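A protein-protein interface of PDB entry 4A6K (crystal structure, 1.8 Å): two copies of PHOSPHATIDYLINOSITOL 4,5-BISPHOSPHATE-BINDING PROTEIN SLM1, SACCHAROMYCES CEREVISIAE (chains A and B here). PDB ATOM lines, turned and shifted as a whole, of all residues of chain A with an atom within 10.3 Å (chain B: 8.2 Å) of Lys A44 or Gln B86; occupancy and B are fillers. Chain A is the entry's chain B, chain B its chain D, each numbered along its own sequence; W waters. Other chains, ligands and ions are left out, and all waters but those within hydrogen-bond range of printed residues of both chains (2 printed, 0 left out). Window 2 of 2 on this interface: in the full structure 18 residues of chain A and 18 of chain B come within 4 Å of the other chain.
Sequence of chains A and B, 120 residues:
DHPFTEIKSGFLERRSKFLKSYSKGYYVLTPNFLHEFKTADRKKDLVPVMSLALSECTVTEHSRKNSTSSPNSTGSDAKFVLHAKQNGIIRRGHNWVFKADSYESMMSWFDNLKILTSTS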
ATOM      1  N   HIS A   2     -17.918 -17.159 -25.387  1.00  0.00           N
ATOM      2  CA  HIS A   2     -18.831 -16.510 -24.364  1.00  0.00           C
ATOM      3  C   HIS A   2     -19.535 -17.480 -23.332  1.00  0.00           C
ATOM      4  O   HIS A   2     -20.162 -18.488 -23.684  1.00  0.00           O
ATOM      5  CB  HIS A   2     -19.714 -15.429 -24.978  1.00  0.00           C
ATOM      6  CG  HIS A   2     -20.829 -15.947 -25.834  1.00  0.00           C
ATOM      7  ND1 HIS A   2     -21.200 -15.330 -27.014  1.00  0.00           N
ATOM      8  CD2 HIS A   2     -21.681 -16.989 -25.672  1.00  0.00           C
ATOM      9  CE1 HIS A   2     -22.239 -15.954 -27.528  1.00  0.00           C
ATOM     10  NE2 HIS A   2     -22.558 -16.958 -26.726  1.00  0.00           N
ATOM     11  N   PRO A   3     -19.360 -17.176 -22.038  1.00  0.00           N
ATOM     12  CA  PRO A   3     -18.927 -18.241 -21.116  1.00  0.00           C
ATOM     13  C   PRO A   3     -20.045 -19.123 -20.600  1.00  0.00           C
ATOM     14  O   PRO A   3     -21.185 -18.737 -20.686  1.00  0.00           O
ATOM     15  CB  PRO A   3     -18.361 -17.446 -19.949  1.00  0.00           C
ATOM     16  CG  PRO A   3     -19.257 -16.239 -19.927  1.00  0.00           C
ATOM     17  CD  PRO A   3     -19.648 -15.917 -21.335  1.00  0.00           C
ATOM     18  N   PHE A   4     -19.694 -20.253 -20.010  1.00  0.00           N
ATOM     19  CA  PHE A   4     -20.694 -21.248 -19.563  1.00  0.00           C
ATOM     20  C   PHE A   4     -19.988 -22.181 -18.589  1.00  0.00           C
ATOM     21  O   PHE A   4     -18.896 -22.696 -18.910  1.00  0.00           O
ATOM     22  CB  PHE A   4     -21.319 -21.974 -20.787  1.00  0.00           C
ATOM     23  CG  PHE A   4     -22.683 -22.616 -20.511  1.00  0.00           C
ATOM     24  CD1 PHE A   4     -22.762 -23.855 -19.933  1.00  0.00           C
ATOM     25  CD2 PHE A   4     -23.889 -21.976 -20.870  1.00  0.00           C
ATOM     26  CE1 PHE A   4     -24.014 -24.489 -19.680  1.00  0.00           C
ATOM     27  CE2 PHE A   4     -25.143 -22.572 -20.599  1.00  0.00           C
ATOM     28  CZ  PHE A   4     -25.217 -23.832 -20.032  1.00  0.00           C
ATOM     29  N   PHE A  37     -29.813 -29.729 -25.728  1.00  0.00           N
ATOM     30  CA  PHE A  37     -30.093 -28.664 -26.765  1.00  0.00           C
ATOM     31  C   PHE A  37     -30.232 -29.391 -28.087  1.00  0.00           C
ATOM     32  O   PHE A  37     -29.704 -30.497 -28.247  1.00  0.00           O
ATOM     33  CB  PHE A  37     -28.960 -27.679 -26.881  1.00  0.00           C
ATOM     34  CG  PHE A  37     -28.690 -26.960 -25.627  1.00  0.00           C
ATOM     35  CD1 PHE A  37     -27.844 -27.494 -24.657  1.00  0.00           C
ATOM     36  CD2 PHE A  37     -29.342 -25.742 -25.403  1.00  0.00           C
ATOM     37  CE1 PHE A  37     -27.618 -26.796 -23.429  1.00  0.00           C
ATOM     38  CE2 PHE A  37     -29.099 -25.025 -24.224  1.00  0.00           C
ATOM     39  CZ  PHE A  37     -28.239 -25.560 -23.235  1.00  0.00           C
ATOM     40  N   LYS A  38     -30.985 -28.826 -29.017  1.00  0.00           N
ATOM     41  CA  LYS A  38     -31.087 -29.503 -30.319  1.00  0.00           C
ATOM     42  C   LYS A  38     -29.770 -29.541 -31.065  1.00  0.00           C
ATOM     43  O   LYS A  38     -29.524 -30.479 -31.827  1.00  0.00           O
ATOM     44  CB  LYS A  38     -32.145 -28.838 -31.196  1.00  0.00           C
ATOM     45  CG  LYS A  38     -33.499 -28.863 -30.579  1.00  0.00           C
ATOM     46  CD  LYS A  38     -34.359 -30.019 -30.994  1.00  0.00           C
ATOM     47  CE  LYS A  38     -35.832 -29.771 -30.681  1.00  0.00           C
ATOM     48  NZ  LYS A  38     -36.538 -31.102 -30.434  1.00  0.00           N
ATOM     49  N   THR A  39     -28.918 -28.523 -30.882  1.00  0.00           N
ATOM     50  CA  THR A  39     -27.699 -28.461 -31.602  1.00  0.00           C
ATOM     51  C   THR A  39     -26.536 -28.063 -30.695  1.00  0.00           C
ATOM     52  O   THR A  39     -26.724 -27.641 -29.534  1.00  0.00           O
ATOM     53  CB  THR A  39     -27.718 -27.401 -32.729  1.00  0.00           C
ATOM     54  OG1 THR A  39     -27.649 -26.087 -32.150  1.00  0.00           O
ATOM     55  CG2 THR A  39     -28.976 -27.542 -33.643  1.00  0.00           C
ATOM     56  N   ALA A  40     -25.359 -28.098 -31.283  1.00  0.00           N
ATOM     57  CA  ALA A  40     -24.149 -27.682 -30.587  1.00  0.00           C
ATOM     58  C   ALA A  40     -23.772 -26.243 -30.693  1.00  0.00           C
ATOM     59  O   ALA A  40     -22.658 -25.874 -30.297  1.00  0.00           O
ATOM     60  CB  ALA A  40     -22.954 -28.606 -30.981  1.00  0.00           C
ATOM     61  N   ASP A  41     -24.651 -25.416 -31.242  1.00  0.00           N
ATOM     62  CA  ASP A  41     -24.344 -24.019 -31.420  1.00  0.00           C
ATOM     63  C   ASP A  41     -24.485 -23.238 -30.059  1.00  0.00           C
ATOM     64  O   ASP A  41     -25.573 -22.804 -29.726  1.00  0.00           O
ATOM     65  CB  ASP A  41     -25.253 -23.410 -32.509  1.00  0.00           C
ATOM     66  CG  ASP A  41     -24.843 -22.009 -32.849  1.00  0.00           C
ATOM     67  OD1 ASP A  41     -24.051 -21.404 -32.092  1.00  0.00           O
ATOM     68  OD2 ASP A  41     -25.260 -21.521 -33.938  1.00  0.00           O
ATOM     69  N   ARG A  42     -23.379 -23.173 -29.321  1.00  0.00           N
ATOM     70  CA  ARG A  42     -23.297 -22.725 -27.909  1.00  0.00           C
ATOM     71  C   ARG A  42     -23.332 -21.215 -27.883  1.00  0.00           C
ATOM     72  O   ARG A  42     -23.410 -20.646 -26.818  1.00  0.00           O
ATOM     73  CB  ARG A  42     -21.999 -23.174 -27.225  1.00  0.00           C
ATOM     74  CG  ARG A  42     -21.668 -24.710 -27.411  1.00  0.00           C
ATOM     75  CD  ARG A  42     -22.755 -25.517 -26.751  1.00  0.00           C
ATOM     76  NE  ARG A  42     -22.898 -25.073 -25.364  1.00  0.00           N
ATOM     77  CZ  ARG A  42     -24.011 -24.650 -24.759  1.00  0.00           C
ATOM     78  NH1 ARG A  42     -25.214 -24.660 -25.361  1.00  0.00           N
ATOM     79  NH2 ARG A  42     -23.920 -24.255 -23.484  1.00  0.00           N
ATOM     80  N   LYS A  43     -23.390 -20.580 -29.057  1.00  0.00           N
ATOM     81  CA  LYS A  43     -23.504 -19.132 -29.125  1.00  0.00           C
ATOM     82  C   LYS A  43     -24.896 -18.699 -29.450  1.00  0.00           C
ATOM     83  O   LYS A  43     -25.272 -17.575 -29.057  1.00  0.00           O
ATOM     84  CB  LYS A  43     -22.511 -18.510 -30.143  1.00  0.00           C
ATOM     85  CG  LYS A  43     -21.065 -19.026 -29.972  1.00  0.00           C
ATOM     86  CD  LYS A  43     -20.021 -18.033 -30.428  1.00  0.00           C
ATOM     87  CE  LYS A  43     -18.790 -18.732 -31.016  1.00  0.00           C
ATOM     88  NZ  LYS A  43     -18.206 -17.881 -32.106  1.00  0.00           N
ATOM     89  N   LYS A  44     -25.691 -19.558 -30.114  1.00  0.00           N
ATOM     90  CA  LYS A  44     -27.048 -19.163 -30.508  1.00  0.00           C
ATOM     91  C   LYS A  44     -28.233 -20.065 -30.038  1.00  0.00           C
ATOM     92  O   LYS A  44     -29.363 -19.591 -29.878  1.00  0.00           O
ATOM     93  CB  LYS A  44     -27.182 -19.013 -32.027  1.00  0.00           C
ATOM     94  CG  LYS A  44     -26.383 -17.923 -32.713  1.00  0.00           C
ATOM     95  CD  LYS A  44     -26.722 -18.021 -34.238  1.00  0.00           C
ATOM     96  CE  LYS A  44     -26.185 -16.850 -35.013  1.00  0.00           C
ATOM     97  NZ  LYS A  44     -24.712 -17.006 -35.290  1.00  0.00           N
ATOM     98  N   ASP A  45     -28.011 -21.355 -29.867  1.00  0.00           N
ATOM     99  CA  ASP A  45     -29.121 -22.288 -29.631  1.00  0.00           C
ATOM    100  C   ASP A  45     -29.061 -22.490 -28.120  1.00  0.00           C
ATOM    101  O   ASP A  45     -28.380 -23.373 -27.610  1.00  0.00           O
ATOM    102  CB  ASP A  45     -28.892 -23.621 -30.381  1.00  0.00           C
ATOM    103  CG  ASP A  45     -29.876 -24.717 -29.977  1.00  0.00           C
ATOM    104  OD1 ASP A  45     -30.944 -24.457 -29.326  1.00  0.00           O
ATOM    105  OD2 ASP A  45     -29.593 -25.892 -30.362  1.00  0.00           O
ATOM    106  N   LEU A  46     -29.663 -21.554 -27.405  1.00  0.00           N
ATOM    107  CA  LEU A  46     -29.439 -21.582 -25.985  1.00  0.00           C
ATOM    108  C   LEU A  46     -30.681 -21.730 -25.104  1.00  0.00           C
ATOM    109  O   LEU A  46     -30.583 -21.481 -23.913  1.00  0.00           O
ATOM    110  CB  LEU A  46     -28.508 -20.421 -25.562  1.00  0.00           C
ATOM    111  CG  LEU A  46     -26.963 -20.562 -25.679  1.00  0.00           C
ATOM    112  CD1 LEU A  46     -26.268 -19.247 -25.457  1.00  0.00           C
ATOM    113  CD2 LEU A  46     -26.301 -21.624 -24.720  1.00  0.00           C
ATOM    114  N   VAL A  47     -31.780 -22.190 -25.672  1.00  0.00           N
ATOM    115  CA  VAL A  47     -32.981 -22.609 -24.892  1.00  0.00           C
ATOM    116  C   VAL A  47     -32.992 -24.141 -24.806  1.00  0.00           C
ATOM    117  O   VAL A  47     -33.124 -24.797 -25.825  1.00  0.00           O
ATOM    118  CB  VAL A  47     -34.241 -22.203 -25.572  1.00  0.00           C
ATOM    119  CG1 VAL A  47     -35.471 -22.599 -24.693  1.00  0.00           C
ATOM    120  CG2 VAL A  47     -34.205 -20.665 -25.855  1.00  0.00           C
ATOM    121  N   PRO A  48     -32.794 -24.707 -23.596  1.00  0.00           N
ATOM    122  CA  PRO A  48     -32.738 -26.177 -23.513  1.00  0.00           C
ATOM    123  C   PRO A  48     -34.016 -26.852 -23.985  1.00  0.00           C
ATOM    124  O   PRO A  48     -35.107 -26.348 -23.707  1.00  0.00           O
ATOM    125  CB  PRO A  48     -32.542 -26.452 -21.987  1.00  0.00           C
ATOM    126  CG  PRO A  48     -31.843 -25.220 -21.502  1.00  0.00           C
ATOM    127  CD  PRO A  48     -32.491 -24.050 -22.309  1.00  0.00           C
ATOM    128  N   ALA B  53     -30.907 -17.753 -21.077  1.00  0.00           N
ATOM    129  CA  ALA B  53     -29.432 -17.767 -21.122  1.00  0.00           C
ATOM    130  C   ALA B  53     -28.806 -16.389 -20.961  1.00  0.00           C
ATOM    131  O   ALA B  53     -29.099 -15.492 -21.710  1.00  0.00           O
ATOM    132  CB  ALA B  53     -28.924 -18.413 -22.473  1.00  0.00           C
ATOM    133  N   LEU B  54     -27.937 -16.260 -19.986  1.00  0.00           N
ATOM    134  CA  LEU B  54     -27.389 -14.941 -19.628  1.00  0.00           C
ATOM    135  C   LEU B  54     -26.485 -14.386 -20.749  1.00  0.00           C
ATOM    136  O   LEU B  54     -26.449 -13.140 -20.973  1.00  0.00           O
ATOM    137  CB  LEU B  54     -26.630 -15.006 -18.335  1.00  0.00           C
ATOM    138  CG  LEU B  54     -27.463 -15.410 -17.112  1.00  0.00           C
ATOM    139  CD1 LEU B  54     -26.552 -15.449 -15.919  1.00  0.00           C
ATOM    140  CD2 LEU B  54     -28.686 -14.481 -16.856  1.00  0.00           C
ATOM    141  N   SER B  55     -25.850 -15.302 -21.497  1.00  0.00           N
ATOM    142  CA  SER B  55     -24.926 -14.832 -22.549  1.00  0.00           C
ATOM    143  C   SER B  55     -25.656 -14.136 -23.723  1.00  0.00           C
ATOM    144  O   SER B  55     -25.022 -13.574 -24.588  1.00  0.00           O
ATOM    145  CB  SER B  55     -24.046 -15.969 -23.048  1.00  0.00           C
ATOM    146  OG  SER B  55     -24.830 -16.876 -23.737  1.00  0.00           O
ATOM    147  N   GLU B  56     -26.970 -14.268 -23.785  1.00  0.00           N
ATOM    148  CA  GLU B  56     -27.824 -13.620 -24.769  1.00  0.00           C
ATOM    149  C   GLU B  56     -28.510 -12.342 -24.276  1.00  0.00           C
ATOM    150  O   GLU B  56     -29.315 -11.733 -25.020  1.00  0.00           O
ATOM    151  CB  GLU B  56     -28.887 -14.611 -25.284  1.00  0.00           C
ATOM    152  CG  GLU B  56     -28.297 -15.806 -25.994  1.00  0.00           C
ATOM    153  CD  GLU B  56     -29.369 -16.806 -26.389  1.00  0.00           C
ATOM    154  OE1 GLU B  56     -30.180 -17.205 -25.532  1.00  0.00           O
ATOM    155  OE2 GLU B  56     -29.420 -17.186 -27.573  1.00  0.00           O
ATOM    156  N   CYS B  57     -28.225 -11.946 -23.037  1.00  0.00           N
ATOM    157  CA  CYS B  57     -28.957 -10.845 -22.318  1.00  0.00           C
ATOM    158  C   CYS B  57     -27.991  -9.755 -21.870  1.00  0.00           C
ATOM    159  O   CYS B  57     -26.798 -10.026 -21.702  1.00  0.00           O
ATOM    160  CB  CYS B  57     -29.648 -11.420 -21.051  1.00  0.00           C
ATOM    161  SG  CYS B  57     -30.953 -12.575 -21.496  1.00  0.00           S
ATOM    162  N   THR B  58     -28.523  -8.546 -21.595  1.00  0.00           N
ATOM    163  CA  THR B  58     -27.784  -7.583 -20.812  1.00  0.00           C
ATOM    164  C   THR B  58     -28.808  -7.009 -19.834  1.00  0.00           C
ATOM    165  O   THR B  58     -30.045  -7.181 -20.060  1.00  0.00           O
ATOM    166  CB  THR B  58     -27.271  -6.463 -21.721  1.00  0.00           C
ATOM    167  OG1 THR B  58     -28.382  -5.923 -22.429  1.00  0.00           O
ATOM    168  CG2 THR B  58     -26.307  -7.026 -22.771  1.00  0.00           C
ATOM    169  N   HIS B  83     -32.522  -7.062 -21.188  1.00  0.00           N
ATOM    170  CA  HIS B  83     -32.598  -6.797 -22.651  1.00  0.00           C
ATOM    171  C   HIS B  83     -32.070  -8.031 -23.406  1.00  0.00           C
ATOM    172  O   HIS B  83     -31.044  -8.564 -23.021  1.00  0.00           O
ATOM    173  CB  HIS B  83     -31.728  -5.570 -23.005  1.00  0.00           C
ATOM    174  CG  HIS B  83     -31.588  -5.340 -24.479  1.00  0.00           C
ATOM    175  ND1 HIS B  83     -32.580  -4.751 -25.240  1.00  0.00           N
ATOM    176  CD2 HIS B  83     -30.578  -5.622 -25.334  1.00  0.00           C
ATOM    177  CE1 HIS B  83     -32.177  -4.672 -26.495  1.00  0.00           C
ATOM    178  NE2 HIS B  83     -30.972  -5.198 -26.578  1.00  0.00           N
ATOM    179  N   ALA B  84     -32.822  -8.534 -24.388  1.00  0.00           N
ATOM    180  CA  ALA B  84     -32.363  -9.658 -25.246  1.00  0.00           C
ATOM    181  C   ALA B  84     -31.436  -9.147 -26.375  1.00  0.00           C
ATOM    182  O   ALA B  84     -31.811  -8.294 -27.194  1.00  0.00           O
ATOM    183  CB  ALA B  84     -33.487 -10.379 -25.832  1.00  0.00           C
ATOM    184  N   LYS B  85     -30.216  -9.658 -26.392  1.00  0.00           N
ATOM    185  CA  LYS B  85     -29.288  -9.384 -27.498  1.00  0.00           C
ATOM    186  C   LYS B  85     -29.506 -10.315 -28.692  1.00  0.00           C
ATOM    187  O   LYS B  85     -29.123  -9.967 -29.807  1.00  0.00           O
ATOM    188  CB  LYS B  85     -27.828  -9.461 -27.044  1.00  0.00           C
ATOM    189  CG  LYS B  85     -27.467  -8.470 -26.017  1.00  0.00           C
ATOM    190  CD  LYS B  85     -25.974  -8.426 -25.850  1.00  0.00           C
ATOM    191  CE  LYS B  85     -25.419  -9.754 -25.320  1.00  0.00           C
ATOM    192  NZ  LYS B  85     -23.961  -9.670 -25.021  1.00  0.00           N
ATOM    193  N   GLN B  86     -30.097 -11.486 -28.454  1.00  0.00           N
ATOM    194  CA  GLN B  86     -30.404 -12.478 -29.491  1.00  0.00           C
ATOM    195  C   GLN B  86     -31.726 -13.131 -29.219  1.00  0.00           C
ATOM    196  O   GLN B  86     -32.227 -13.069 -28.068  1.00  0.00           O
ATOM    197  CB  GLN B  86     -29.372 -13.603 -29.504  1.00  0.00           C
ATOM    198  CG  GLN B  86     -27.954 -13.157 -29.399  1.00  0.00           C
ATOM    199  CD  GLN B  86     -27.079 -14.322 -28.940  1.00  0.00           C
ATOM    200  OE1 GLN B  86     -27.388 -15.487 -29.255  1.00  0.00           O
ATOM    201  NE2 GLN B  86     -26.012 -14.023 -28.182  1.00  0.00           N
ATOM    202  N   ASN B  87     -32.266 -13.763 -30.268  1.00  0.00           N
ATOM    203  CA  ASN B  87     -33.506 -14.481 -30.234  1.00  0.00           C
ATOM    204  C   ASN B  87     -33.355 -15.710 -29.337  1.00  0.00           C
ATOM    205  O   ASN B  87     -32.523 -16.588 -29.599  1.00  0.00           O
ATOM    206  CB  ASN B  87     -33.887 -14.973 -31.629  1.00  0.00           C
ATOM    207  CG  ASN B  87     -34.463 -13.877 -32.509  1.00  0.00           C
ATOM    208  OD1 ASN B  87     -34.077 -13.744 -33.696  1.00  0.00           O
ATOM    209  ND2 ASN B  87     -35.406 -13.118 -31.975  1.00  0.00           N
ATOM    210  N   GLY B  88     -34.137 -15.770 -28.280  1.00  0.00           N
ATOM    211  CA  GLY B  88     -34.117 -16.964 -27.428  1.00  0.00           C
ATOM    212  C   GLY B  88     -35.524 -17.129 -26.942  1.00  0.00           C
ATOM    213  O   GLY B  88     -36.444 -17.321 -27.713  1.00  0.00           O
ATOM    214  N   ILE B  89     -35.699 -17.062 -25.636  1.00  0.00           N
ATOM    215  CA  ILE B  89     -37.025 -16.952 -25.098  1.00  0.00           C
ATOM    216  C   ILE B  89     -37.628 -15.581 -25.381  1.00  0.00           C
ATOM    217  O   ILE B  89     -38.815 -15.468 -25.605  1.00  0.00           O
ATOM    218  CB  ILE B  89     -37.007 -17.184 -23.626  1.00  0.00           C
ATOM    219  CG1 ILE B  89     -36.874 -18.713 -23.400  1.00  0.00           C
ATOM    220  CG2 ILE B  89     -38.285 -16.648 -23.018  1.00  0.00           C
ATOM    221  CD1 ILE B  89     -35.952 -18.945 -22.327  1.00  0.00           C
ATOM    222  N   ILE B  90     -36.794 -14.563 -25.363  1.00  0.00           N
ATOM    223  CA  ILE B  90     -37.174 -13.189 -25.698  1.00  0.00           C
ATOM    224  C   ILE B  90     -36.722 -12.912 -27.174  1.00  0.00           C
ATOM    225  O   ILE B  90     -35.661 -13.410 -27.577  1.00  0.00           O
ATOM    226  CB  ILE B  90     -36.433 -12.249 -24.713  1.00  0.00           C
ATOM    227  CG1 ILE B  90     -36.688 -12.658 -23.238  1.00  0.00           C
ATOM    228  CG2 ILE B  90     -36.797 -10.767 -24.931  1.00  0.00           C
ATOM    229  CD1 ILE B  90     -36.004 -11.724 -22.192  1.00  0.00           C
ATOM    230  N   ARG B  91     -37.500 -12.149 -27.961  1.00  0.00           N
ATOM    231  CA  ARG B  91     -37.068 -11.733 -29.337  1.00  0.00           C
ATOM    232  C   ARG B  91     -35.882 -10.800 -29.228  1.00  0.00           C
ATOM    233  O   ARG B  91     -35.825 -10.013 -28.282  1.00  0.00           O
ATOM    234  CB  ARG B  91     -38.227 -11.044 -30.122  1.00  0.00           C
ATOM    235  CG  ARG B  91     -39.057 -12.009 -30.940  1.00  0.00           C
ATOM    236  N   ARG B  92     -34.935 -10.873 -30.176  1.00  0.00           N
ATOM    237  CA  ARG B  92     -33.791  -9.978 -30.187  1.00  0.00           C
ATOM    238  C   ARG B  92     -34.274  -8.523 -30.213  1.00  0.00           C
ATOM    239  O   ARG B  92     -35.242  -8.212 -30.895  1.00  0.00           O
ATOM    240  CB  ARG B  92     -32.870 -10.240 -31.417  1.00  0.00           C
ATOM    241  CG  ARG B  92     -31.790  -9.177 -31.634  1.00  0.00           C
ATOM    242  CD  ARG B  92     -31.573  -8.839 -33.166  1.00  0.00           C
ATOM    243  NE  ARG B  92     -30.233  -9.153 -33.651  1.00  0.00           N
ATOM    244  N   GLY B  93     -33.597  -7.688 -29.450  1.00  0.00           N
ATOM    245  CA  GLY B  93     -33.914  -6.286 -29.255  1.00  0.00           C
ATOM    246  C   GLY B  93     -34.999  -6.005 -28.242  1.00  0.00           C
ATOM    247  O   GLY B  93     -35.228  -4.860 -27.945  1.00  0.00           O
ATOM    248  N   HIS B  94     -35.708  -7.032 -27.752  1.00  0.00           N
ATOM    249  CA  HIS B  94     -36.815  -6.810 -26.834  1.00  0.00           C
ATOM    250  C   HIS B  94     -36.378  -6.841 -25.347  1.00  0.00           C
ATOM    251  O   HIS B  94     -35.240  -7.210 -25.017  1.00  0.00           O
ATOM    252  CB  HIS B  94     -37.946  -7.825 -27.082  1.00  0.00           C
ATOM    253  CG  HIS B  94     -38.715  -7.594 -28.349  1.00  0.00           C
ATOM    254  ND1 HIS B  94     -40.089  -7.743 -28.422  1.00  0.00           N
ATOM    255  CD2 HIS B  94     -38.307  -7.236 -29.595  1.00  0.00           C
ATOM    256  CE1 HIS B  94     -40.492  -7.494 -29.659  1.00  0.00           C
ATOM    257  NE2 HIS B  94     -39.430  -7.181 -30.390  1.00  0.00           N
HETATM  258  O   HOH W   1     -32.450 -19.362 -23.097  1.00  0.00           O
HETATM  259  O   HOH W   2     -32.768 -20.023 -29.437  1.00  0.00           O
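Of the 18 printed residues of chain B, 6 touch a printed residue of chain A. Hydrophobic or aromatic side chains of chain B that line the printed part of chain A: Ala B53. Along chain B the printed residues that touch a printed residue of chain A span positions 53 to 89. Printed residues of chain A that touch a printed residue of chain B: His A2, Lys A43, Lys A44, Leu A46 and Val A47. Hydrophobic or aromatic side chains of chain A within 4 Å of the printed part of chain B: His A2, Leu A46 and Val A47. Among the printed residues, no Asp or Glu carboxylate lies within 4 Å of a Lys or Arg side-chain nitrogen of the other chain.
Water W1 lies within hydrogen-bond range of the backbone carbonyl oxygen of Leu A46 (2.9 Å) and the backbone NH of Ala B53 (3.0 Å). Water W2 lies within hydrogen-bond range of O of Asn B87 (3.4 Å) and O of Lys A44 (3.5 Å).
Lys A44 touches just these residues of chain B: Glu B56 and Gln B86. Of chain A, only Lys A43 and Lys A44 come within 4 Å of Gln B86. Glu B56 touches two residues of chain A. No residue of chain A comes within 4 Å of Lys B85. No residue of chain A comes within 4 Å of Asn B87. Gly B88 touches just one residue of chain A: Val A47. Of the printed residues of chain B, Lys A43 touches Gln B86 (3.0 Å). Of the printed residues of chain B, Val A47 touches Gly B88 (3.9 Å) and Ile B89 (3.9 Å). The nearest residue of chain A that does not touch Gln B86 is His A2 (4.3 Å).
No position is printed for both chains. Of the 9 pairs that touch across the chains among the printed residues, none has its exchanged pair printed and touching as well.
Among the printed residues, merely in contact across the chains: Leu A46 with Ser B55 (3.3 Å), Leu A46 with Glu B56 (3.6 Å), His A2 with Ser B55 (3.7 Å), Leu A46 with Ala B53 (3.7 Å), Lys A44 with Gln B86 (3.9 Å), Val A47 with Ile B89 (3.9 Å) and Val A47 with Gly B88 (3.9 Å).
O of Glu B56 is in hydrogen-bond range of N of Lys B85 (2.6 Å). The side-chain carboxylate (OD1) of Asp A41 lies within hydrogen-bond range of the backbone NH (N) of Lys A44. OE2 of Glu B56 lies close to OE1 of Gln B86 (3.1 Å). The side-chain carboxylate (OD1) of Asp A41 lies close to the backbone NH (N) of Lys A43 (3.2 Å). The backbone carbonyl oxygen (O) of Ala B53 is in hydrogen-bond range of the side-chain sulfur (SG) of Cys B57 (3.5 Å).
O of Lys A43 sits close to OE1 of Gln B86 (3.0 Å). The side-chain carboxylate (OE2) of Glu B56 lies close to the backbone carbonyl oxygen (O) of Lys A44, 3.3 Å away.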
